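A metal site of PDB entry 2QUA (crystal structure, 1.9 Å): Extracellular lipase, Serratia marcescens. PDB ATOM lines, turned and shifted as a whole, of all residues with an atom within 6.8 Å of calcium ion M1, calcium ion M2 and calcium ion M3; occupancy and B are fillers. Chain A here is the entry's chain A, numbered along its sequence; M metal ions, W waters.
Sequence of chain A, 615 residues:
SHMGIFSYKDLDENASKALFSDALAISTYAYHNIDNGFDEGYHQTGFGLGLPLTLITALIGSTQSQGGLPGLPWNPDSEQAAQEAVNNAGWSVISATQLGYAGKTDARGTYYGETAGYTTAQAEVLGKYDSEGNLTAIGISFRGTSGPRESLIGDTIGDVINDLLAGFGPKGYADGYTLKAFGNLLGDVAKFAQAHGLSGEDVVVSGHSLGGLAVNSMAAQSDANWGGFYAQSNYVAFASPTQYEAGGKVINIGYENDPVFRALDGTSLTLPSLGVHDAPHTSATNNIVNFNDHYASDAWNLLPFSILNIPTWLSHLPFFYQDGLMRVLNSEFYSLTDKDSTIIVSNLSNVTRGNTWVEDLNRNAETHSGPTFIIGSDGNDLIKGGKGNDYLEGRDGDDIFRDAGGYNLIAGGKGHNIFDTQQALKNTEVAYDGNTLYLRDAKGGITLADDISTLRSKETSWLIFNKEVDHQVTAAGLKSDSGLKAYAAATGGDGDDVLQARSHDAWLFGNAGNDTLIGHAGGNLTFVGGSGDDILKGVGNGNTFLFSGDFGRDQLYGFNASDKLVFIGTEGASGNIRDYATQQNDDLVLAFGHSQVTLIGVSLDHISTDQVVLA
The backbone NH (N) of Gly 510 lies within hydrogen-bond range of the backbone carbonyl oxygen (O) of Val 528, 3.0 Å away.
The backbone carbonyl oxygen (O) of Gly 492 is in hydrogen-bond range of the side-chain amide nitrogen (ND2) of Asn 511, 2.7 Å away.
The backbone NH (N) of Asp 554 is in hydrogen-bond range of the backbone carbonyl oxygen (O) of Gln 596 (2.9 Å).
The nearest printed residue that does not touch calcium ion M1 is Gly 530 (4.01 Å).
Seven residues have an atom within 4 Å of calcium ion M2: Gly 493, Gly 495, Asp 497, Gly 510, Asn 511, Ala 512 and Asp 515.
The nearest printed residue that does not touch calcium ion M2 is Asp 494 (4.1 Å).
Of the 30 residues printed, 6 come within 4 Å of calcium ion M3.
The side-chain carboxylate (OD2) of Asp 515 is bound to calcium ion M1 (2.3 Å).
Calcium ion M1 is bound by O of Asn 511 (2.3 Å).
Calcium ion M1 is bound by the backbone carbonyl oxygen (O) of Ser 531, at 2.3 Å.
Calcium ion M1 is bound by OD1 of Asp 534 (2.3 Å).
Calcium ion M1 is bound by O of Gly 529, at 2.4 Å.
Calcium ion M1 is bound by the backbone carbonyl oxygen (O) of Gly 513, at 2.4 Å.
Calcium ion M1 has six donor atoms within binding distance.
Slightly farther from calcium ion M1 lies OD2 of Asp 534 (3.0 Å).
Calcium ion M2 is bound by the backbone carbonyl oxygen (O) of Ala 512 (2.3 Å), the side-chain carboxylate (OD1) of Asp 515 (2.3 Å), the side-chain carboxylate (OD2) of Asp 497 (2.3 Å), the backbone carbonyl oxygen (O) of Gly 493 (2.3 Å), the backbone carbonyl oxygen (O) of Gly 510 (2.3 Å) and the backbone carbonyl oxygen (O) of Gly 495 (2.4 Å).
Calcium ion M2 has six donor atoms within binding distance.
Slightly farther from calcium ion M2 lies OD2 of Asp 515 (2.9 Å).
Calcium ion M3 is bound by O of Phe 551 (2.3 Å), OD2 of Asp 534 (2.3 Å), water W1 (2.3 Å), O of Gly 530 (2.3 Å), O of Gly 532 (2.4 Å) and OD1 of Asp 554 (2.4 Å).
Calcium ion M3 has six donor atoms within binding distance.
Water W1 bridges the side-chain carboxylate (OD2) of Asp 554 (2.5 Å) and the backbone NH (N) of Gly 530 (3.4 Å).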
ATOM      1  N   GLY A 492      31.641  23.081 -11.653  1.00  0.00           N
ATOM      2  CA  GLY A 492      32.067  22.973 -10.250  1.00  0.00           C
ATOM      3  C   GLY A 492      32.243  21.519  -9.831  1.00  0.00           C
ATOM      4  O   GLY A 492      32.169  20.609 -10.662  1.00  0.00           O
ATOM      5  N   GLY A 493      32.480  21.313  -8.533  1.00  0.00           N
ATOM      6  CA  GLY A 493      32.639  19.981  -7.958  1.00  0.00           C
ATOM      7  C   GLY A 493      31.737  19.766  -6.752  1.00  0.00           C
ATOM      8  O   GLY A 493      30.684  20.392  -6.639  1.00  0.00           O
ATOM      9  N   ASP A 494      32.174  18.897  -5.837  1.00  0.00           N
ATOM     10  CA  ASP A 494      31.423  18.554  -4.631  1.00  0.00           C
ATOM     11  C   ASP A 494      31.200  19.737  -3.686  1.00  0.00           C
ATOM     12  O   ASP A 494      30.294  19.724  -2.855  1.00  0.00           O
ATOM     13  CB  ASP A 494      32.131  17.444  -3.863  1.00  0.00           C
ATOM     14  CG  ASP A 494      32.030  16.089  -4.550  1.00  0.00           C
ATOM     15  OD1 ASP A 494      31.099  15.912  -5.366  1.00  0.00           O
ATOM     16  OD2 ASP A 494      32.868  15.204  -4.266  1.00  0.00           O
ATOM     17  N   GLY A 495      32.059  20.744  -3.823  1.00  0.00           N
ATOM     18  CA  GLY A 495      32.026  21.896  -2.915  1.00  0.00           C
ATOM     19  C   GLY A 495      30.935  22.896  -3.238  1.00  0.00           C
ATOM     20  O   GLY A 495      30.236  22.786  -4.246  1.00  0.00           O
ATOM     21  N   ASP A 496      30.793  23.879  -2.365  1.00  0.00           N
ATOM     22  CA  ASP A 496      29.894  24.989  -2.557  1.00  0.00           C
ATOM     23  C   ASP A 496      30.641  25.968  -3.451  1.00  0.00           C
ATOM     24  O   ASP A 496      31.394  26.815  -2.970  1.00  0.00           O
ATOM     25  CB  ASP A 496      29.539  25.618  -1.202  1.00  0.00           C
ATOM     26  CG  ASP A 496      28.923  24.607  -0.229  1.00  0.00           C
ATOM     27  OD1 ASP A 496      28.416  23.556  -0.685  1.00  0.00           O
ATOM     28  OD2 ASP A 496      28.941  24.859   0.985  1.00  0.00           O
ATOM     29  N   ASP A 497      30.425  25.839  -4.757  1.00  0.00           N
ATOM     30  CA  ASP A 497      31.187  26.590  -5.748  1.00  0.00           C
ATOM     31  C   ASP A 497      30.537  27.922  -6.125  1.00  0.00           C
ATOM     32  O   ASP A 497      29.309  28.037  -6.188  1.00  0.00           O
ATOM     33  CB  ASP A 497      31.340  25.744  -7.011  1.00  0.00           C
ATOM     34  CG  ASP A 497      31.928  24.377  -6.723  1.00  0.00           C
ATOM     35  OD1 ASP A 497      33.041  24.331  -6.165  1.00  0.00           O
ATOM     36  OD2 ASP A 497      31.279  23.365  -7.051  1.00  0.00           O
ATOM     37  N   LEU A 499      30.352  30.050  -9.386  1.00  0.00           N
ATOM     38  CA  LEU A 499      30.625  29.983 -10.817  1.00  0.00           C
ATOM     39  C   LEU A 499      30.155  31.227 -11.556  1.00  0.00           C
ATOM     40  O   LEU A 499      28.947  31.464 -11.674  1.00  0.00           O
ATOM     41  CB  LEU A 499      29.949  28.747 -11.429  1.00  0.00           C
ATOM     42  CG  LEU A 499      30.357  27.407 -10.829  1.00  0.00           C
ATOM     43  CD1 LEU A 499      29.640  26.254 -11.517  1.00  0.00           C
ATOM     44  CD2 LEU A 499      31.859  27.263 -10.931  1.00  0.00           C
ATOM     45  N   PHE A 509      27.473  24.254 -14.478  1.00  0.00           N
ATOM     46  CA  PHE A 509      27.161  23.060 -13.703  1.00  0.00           C
ATOM     47  C   PHE A 509      27.706  23.208 -12.281  1.00  0.00           C
ATOM     48  O   PHE A 509      28.920  23.170 -12.076  1.00  0.00           O
ATOM     49  CB  PHE A 509      27.807  21.835 -14.349  1.00  0.00           C
ATOM     50  CG  PHE A 509      27.342  21.551 -15.762  1.00  0.00           C
ATOM     51  CD1 PHE A 509      26.022  21.187 -16.022  1.00  0.00           C
ATOM     52  CD2 PHE A 509      28.226  21.647 -16.826  1.00  0.00           C
ATOM     53  CE1 PHE A 509      25.606  20.914 -17.334  1.00  0.00           C
ATOM     54  CE2 PHE A 509      27.820  21.374 -18.128  1.00  0.00           C
ATOM     55  CZ  PHE A 509      26.511  21.013 -18.368  1.00  0.00           C
ATOM     56  N   GLY A 510      26.819  23.390 -11.307  1.00  0.00           N
ATOM     57  CA  GLY A 510      27.238  23.499  -9.923  1.00  0.00           C
ATOM     58  C   GLY A 510      27.656  22.146  -9.362  1.00  0.00           C
ATOM     59  O   GLY A 510      28.560  22.078  -8.545  1.00  0.00           O
ATOM     60  N   ASN A 511      26.986  21.082  -9.819  1.00  0.00           N
ATOM     61  CA  ASN A 511      27.183  19.728  -9.272  1.00  0.00           C
ATOM     62  C   ASN A 511      26.782  19.700  -7.798  1.00  0.00           C
ATOM     63  O   ASN A 511      25.940  20.496  -7.384  1.00  0.00           O
ATOM     64  CB  ASN A 511      28.631  19.223  -9.517  1.00  0.00           C
ATOM     65  CG  ASN A 511      28.868  18.809 -10.989  1.00  0.00           C
ATOM     66  OD1 ASN A 511      28.000  18.222 -11.618  1.00  0.00           O
ATOM     67  ND2 ASN A 511      30.046  19.118 -11.526  1.00  0.00           N
ATOM     68  N   ALA A 512      27.348  18.813  -7.006  1.00  0.00           N
ATOM     69  CA  ALA A 512      26.926  18.700  -5.602  1.00  0.00           C
ATOM     70  C   ALA A 512      27.263  19.948  -4.802  1.00  0.00           C
ATOM     71  O   ALA A 512      28.073  20.781  -5.220  1.00  0.00           O
ATOM     72  CB  ALA A 512      27.537  17.474  -4.950  1.00  0.00           C
ATOM     73  N   GLY A 513      26.642  20.084  -3.633  1.00  0.00           N
ATOM     74  CA  GLY A 513      26.896  21.239  -2.784  1.00  0.00           C
ATOM     75  C   GLY A 513      26.020  22.424  -3.153  1.00  0.00           C
ATOM     76  O   GLY A 513      25.253  22.388  -4.134  1.00  0.00           O
ATOM     77  N   ASN A 514      26.142  23.472  -2.366  1.00  0.00           N
ATOM     78  CA  ASN A 514      25.327  24.674  -2.529  1.00  0.00           C
ATOM     79  C   ASN A 514      26.105  25.718  -3.333  1.00  0.00           C
ATOM     80  O   ASN A 514      26.971  26.416  -2.808  1.00  0.00           O
ATOM     81  CB  ASN A 514      24.868  25.182  -1.155  1.00  0.00           C
ATOM     82  CG  ASN A 514      24.023  24.144  -0.413  1.00  0.00           C
ATOM     83  OD1 ASN A 514      23.669  23.091  -0.958  1.00  0.00           O
ATOM     84  ND2 ASN A 514      23.685  24.450   0.831  1.00  0.00           N
ATOM     85  N   ASP A 515      25.774  25.799  -4.612  1.00  0.00           N
ATOM     86  CA  ASP A 515      26.530  26.595  -5.568  1.00  0.00           C
ATOM     87  C   ASP A 515      25.862  27.914  -5.939  1.00  0.00           C
ATOM     88  O   ASP A 515      24.625  28.037  -5.894  1.00  0.00           O
ATOM     89  CB  ASP A 515      26.691  25.761  -6.848  1.00  0.00           C
ATOM     90  CG  ASP A 515      27.327  24.393  -6.585  1.00  0.00           C
ATOM     91  OD1 ASP A 515      28.468  24.363  -6.114  1.00  0.00           O
ATOM     92  OD2 ASP A 515      26.672  23.360  -6.861  1.00  0.00           O
ATOM     93  N   LEU A 517      25.608  30.301  -9.176  1.00  0.00           N
ATOM     94  CA  LEU A 517      25.810  30.386 -10.624  1.00  0.00           C
ATOM     95  C   LEU A 517      25.383  31.755 -11.136  1.00  0.00           C
ATOM     96  O   LEU A 517      24.212  32.138 -10.993  1.00  0.00           O
ATOM     97  CB  LEU A 517      25.015  29.292 -11.353  1.00  0.00           C
ATOM     98  CG  LEU A 517      25.495  27.839 -11.335  1.00  0.00           C
ATOM     99  CD1 LEU A 517      25.825  27.361  -9.936  1.00  0.00           C
ATOM    100  CD2 LEU A 517      24.445  26.912 -11.973  1.00  0.00           C
ATOM    101  N   VAL A 528      22.512  24.861 -14.406  1.00  0.00           N
ATOM    102  CA  VAL A 528      22.203  23.577 -13.811  1.00  0.00           C
ATOM    103  C   VAL A 528      22.809  23.545 -12.413  1.00  0.00           C
ATOM    104  O   VAL A 528      24.011  23.254 -12.260  1.00  0.00           O
ATOM    105  CB  VAL A 528      22.813  22.448 -14.627  1.00  0.00           C
ATOM    106  CG1 VAL A 528      22.265  21.103 -14.138  1.00  0.00           C
ATOM    107  CG2 VAL A 528      22.561  22.667 -16.117  1.00  0.00           C
ATOM    108  N   GLY A 529      22.023  23.859 -11.386  1.00  0.00           N
ATOM    109  CA  GLY A 529      22.605  23.929 -10.032  1.00  0.00           C
ATOM    110  C   GLY A 529      23.033  22.560  -9.519  1.00  0.00           C
ATOM    111  O   GLY A 529      23.966  22.434  -8.713  1.00  0.00           O
ATOM    112  N   GLY A 530      22.351  21.529 -10.023  1.00  0.00           N
ATOM    113  CA  GLY A 530      22.613  20.151  -9.657  1.00  0.00           C
ATOM    114  C   GLY A 530      22.011  19.881  -8.289  1.00  0.00           C
ATOM    115  O   GLY A 530      21.154  20.633  -7.832  1.00  0.00           O
ATOM    116  N   SER A 531      22.459  18.825  -7.643  1.00  0.00           N
ATOM    117  CA  SER A 531      22.003  18.558  -6.288  1.00  0.00           C
ATOM    118  C   SER A 531      22.514  19.664  -5.363  1.00  0.00           C
ATOM    119  O   SER A 531      23.367  20.476  -5.754  1.00  0.00           O
ATOM    120  CB  SER A 531      22.464  17.180  -5.808  1.00  0.00           C
ATOM    121  OG  SER A 531      23.846  17.188  -5.528  1.00  0.00           O
ATOM    122  N   GLY A 532      21.985  19.700  -4.148  1.00  0.00           N
ATOM    123  CA  GLY A 532      22.273  20.785  -3.205  1.00  0.00           C
ATOM    124  C   GLY A 532      21.383  21.989  -3.472  1.00  0.00           C
ATOM    125  O   GLY A 532      20.622  22.060  -4.456  1.00  0.00           O
ATOM    126  N   ASP A 533      21.480  22.964  -2.584  1.00  0.00           N
ATOM    127  CA  ASP A 533      20.629  24.142  -2.634  1.00  0.00           C
ATOM    128  C   ASP A 533      21.388  25.288  -3.252  1.00  0.00           C
ATOM    129  O   ASP A 533      22.296  25.837  -2.632  1.00  0.00           O
ATOM    130  CB  ASP A 533      20.156  24.507  -1.240  1.00  0.00           C
ATOM    131  CG  ASP A 533      19.415  23.365  -0.571  1.00  0.00           C
ATOM    132  OD1 ASP A 533      18.912  22.471  -1.283  1.00  0.00           O
ATOM    133  OD2 ASP A 533      19.319  23.362   0.678  1.00  0.00           O
ATOM    134  N   ASP A 534      20.998  25.634  -4.478  1.00  0.00           N
ATOM    135  CA  ASP A 534      21.793  26.539  -5.321  1.00  0.00           C
ATOM    136  C   ASP A 534      21.131  27.903  -5.569  1.00  0.00           C
ATOM    137  O   ASP A 534      19.920  28.054  -5.540  1.00  0.00           O
ATOM    138  CB  ASP A 534      22.089  25.858  -6.670  1.00  0.00           C
ATOM    139  CG  ASP A 534      22.717  24.471  -6.508  1.00  0.00           C
ATOM    140  OD1 ASP A 534      23.874  24.376  -6.053  1.00  0.00           O
ATOM    141  OD2 ASP A 534      22.056  23.463  -6.815  1.00  0.00           O
ATOM    142  N   LEU A 536      20.782  30.837  -8.370  1.00  0.00           N
ATOM    143  CA  LEU A 536      20.868  31.005  -9.824  1.00  0.00           C
ATOM    144  C   LEU A 536      20.586  32.449 -10.228  1.00  0.00           C
ATOM    145  O   LEU A 536      19.443  32.925 -10.140  1.00  0.00           O
ATOM    146  CB  LEU A 536      19.892  30.070 -10.552  1.00  0.00           C
ATOM    147  CG  LEU A 536      19.791  28.664  -9.955  1.00  0.00           C
ATOM    148  CD1 LEU A 536      18.543  27.924 -10.527  1.00  0.00           C
ATOM    149  CD2 LEU A 536      21.089  27.851 -10.160  1.00  0.00           C
ATOM    150  N   PHE A 547      16.463  21.570 -14.181  1.00  0.00           N
ATOM    151  CA  PHE A 547      16.315  20.848 -12.917  1.00  0.00           C
ATOM    152  C   PHE A 547      15.909  19.419 -13.204  1.00  0.00           C
ATOM    153  O   PHE A 547      14.976  19.197 -13.988  1.00  0.00           O
ATOM    154  CB  PHE A 547      15.210  21.479 -12.067  1.00  0.00           C
ATOM    155  CG  PHE A 547      15.340  22.967 -11.935  1.00  0.00           C
ATOM    156  CD1 PHE A 547      16.045  23.505 -10.876  1.00  0.00           C
ATOM    157  CD2 PHE A 547      14.775  23.818 -12.875  1.00  0.00           C
ATOM    158  CE1 PHE A 547      16.187  24.899 -10.747  1.00  0.00           C
ATOM    159  CE2 PHE A 547      14.911  25.219 -12.761  1.00  0.00           C
ATOM    160  CZ  PHE A 547      15.613  25.754 -11.688  1.00  0.00           C
ATOM    161  N   ASP A 550      16.254  14.710  -7.885  1.00  0.00           N
ATOM    162  CA  ASP A 550      16.215  15.460  -6.645  1.00  0.00           C
ATOM    163  C   ASP A 550      17.183  16.641  -6.736  1.00  0.00           C
ATOM    164  O   ASP A 550      18.365  16.517  -6.413  1.00  0.00           O
ATOM    165  CB  ASP A 550      16.512  14.556  -5.448  1.00  0.00           C
ATOM    166  CG  ASP A 550      15.489  13.409  -5.323  1.00  0.00           C
ATOM    167  OD1 ASP A 550      14.268  13.707  -5.281  1.00  0.00           O
ATOM    168  OD2 ASP A 550      15.904  12.226  -5.275  1.00  0.00           O
ATOM    169  N   PHE A 551      16.677  17.790  -7.178  1.00  0.00           N
ATOM    170  CA  PHE A 551      17.536  18.933  -7.440  1.00  0.00           C
ATOM    171  C   PHE A 551      17.681  19.897  -6.245  1.00  0.00           C
ATOM    172  O   PHE A 551      18.211  20.978  -6.408  1.00  0.00           O
ATOM    173  CB  PHE A 551      17.086  19.681  -8.718  1.00  0.00           C
ATOM    174  CG  PHE A 551      15.693  20.239  -8.633  1.00  0.00           C
ATOM    175  CD1 PHE A 551      14.597  19.463  -9.038  1.00  0.00           C
ATOM    176  CD2 PHE A 551      15.457  21.535  -8.154  1.00  0.00           C
ATOM    177  CE1 PHE A 551      13.302  19.967  -8.959  1.00  0.00           C
ATOM    178  CE2 PHE A 551      14.162  22.043  -8.066  1.00  0.00           C
ATOM    179  CZ  PHE A 551      13.076  21.263  -8.470  1.00  0.00           C
ATOM    180  N   GLY A 552      17.227  19.495  -5.062  1.00  0.00           N
ATOM    181  CA  GLY A 552      17.357  20.336  -3.855  1.00  0.00           C
ATOM    182  C   GLY A 552      16.495  21.584  -3.902  1.00  0.00           C
ATOM    183  O   GLY A 552      15.523  21.645  -4.655  1.00  0.00           O
ATOM    184  N   ARG A 553      16.845  22.600  -3.109  1.00  0.00           N
ATOM    185  CA  ARG A 553      16.000  23.773  -3.038  1.00  0.00           C
ATOM    186  C   ARG A 553      16.715  25.021  -3.543  1.00  0.00           C
ATOM    187  O   ARG A 553      17.550  25.579  -2.832  1.00  0.00           O
ATOM    188  CB  ARG A 553      15.538  23.987  -1.588  1.00  0.00           C
ATOM    189  CG  ARG A 553      14.831  22.759  -0.983  1.00  0.00           C
ATOM    190  CD  ARG A 553      14.151  23.100   0.363  1.00  0.00           C
ATOM    191  NE  ARG A 553      13.750  21.890   1.087  1.00  0.00           N
ATOM    192  CZ  ARG A 553      12.665  21.147   0.810  1.00  0.00           C
ATOM    193  NH1 ARG A 553      11.853  21.479  -0.198  1.00  0.00           N
ATOM    194  NH2 ARG A 553      12.393  20.070   1.540  1.00  0.00           N
ATOM    195  N   ASP A 554      16.374  25.453  -4.745  1.00  0.00           N
ATOM    196  CA  ASP A 554      17.095  26.530  -5.417  1.00  0.00           C
ATOM    197  C   ASP A 554      16.385  27.889  -5.274  1.00  0.00           C
ATOM    198  O   ASP A 554      15.173  27.941  -5.069  1.00  0.00           O
ATOM    199  CB  ASP A 554      17.207  26.220  -6.913  1.00  0.00           C
ATOM    200  CG  ASP A 554      18.277  25.146  -7.268  1.00  0.00           C
ATOM    201  OD1 ASP A 554      18.736  24.330  -6.422  1.00  0.00           O
ATOM    202  OD2 ASP A 554      18.683  25.140  -8.453  1.00  0.00           O
ATOM    203  N   GLN A 596      12.626  22.205  -4.810  1.00  0.00           N
ATOM    204  CA  GLN A 596      11.770  23.328  -5.132  1.00  0.00           C
ATOM    205  C   GLN A 596      12.596  24.407  -5.736  1.00  0.00           C
ATOM    206  O   GLN A 596      13.824  24.406  -5.592  1.00  0.00           O
ATOM    207  CB  GLN A 596      11.069  23.861  -3.868  1.00  0.00           C
ATOM    208  CG  GLN A 596      11.963  24.707  -2.983  1.00  0.00           C
ATOM    209  CD  GLN A 596      11.271  25.187  -1.719  1.00  0.00           C
ATOM    210  OE1 GLN A 596      10.572  24.420  -1.044  1.00  0.00           O
ATOM    211  NE2 GLN A 596      11.454  26.465  -1.378  1.00  0.00           N
HETATM  212 CA    CA M   1      24.711  22.224  -6.470  1.00  0.00          CA
HETATM  213 CA    CA M   2      29.368  22.267  -6.375  1.00  0.00          CA
HETATM  214 CA    CA M   3      20.021  22.358  -6.717  1.00  0.00          CA
HETATM  215  O   HOH W   1      19.405  22.799  -8.930  1.00  0.00           O
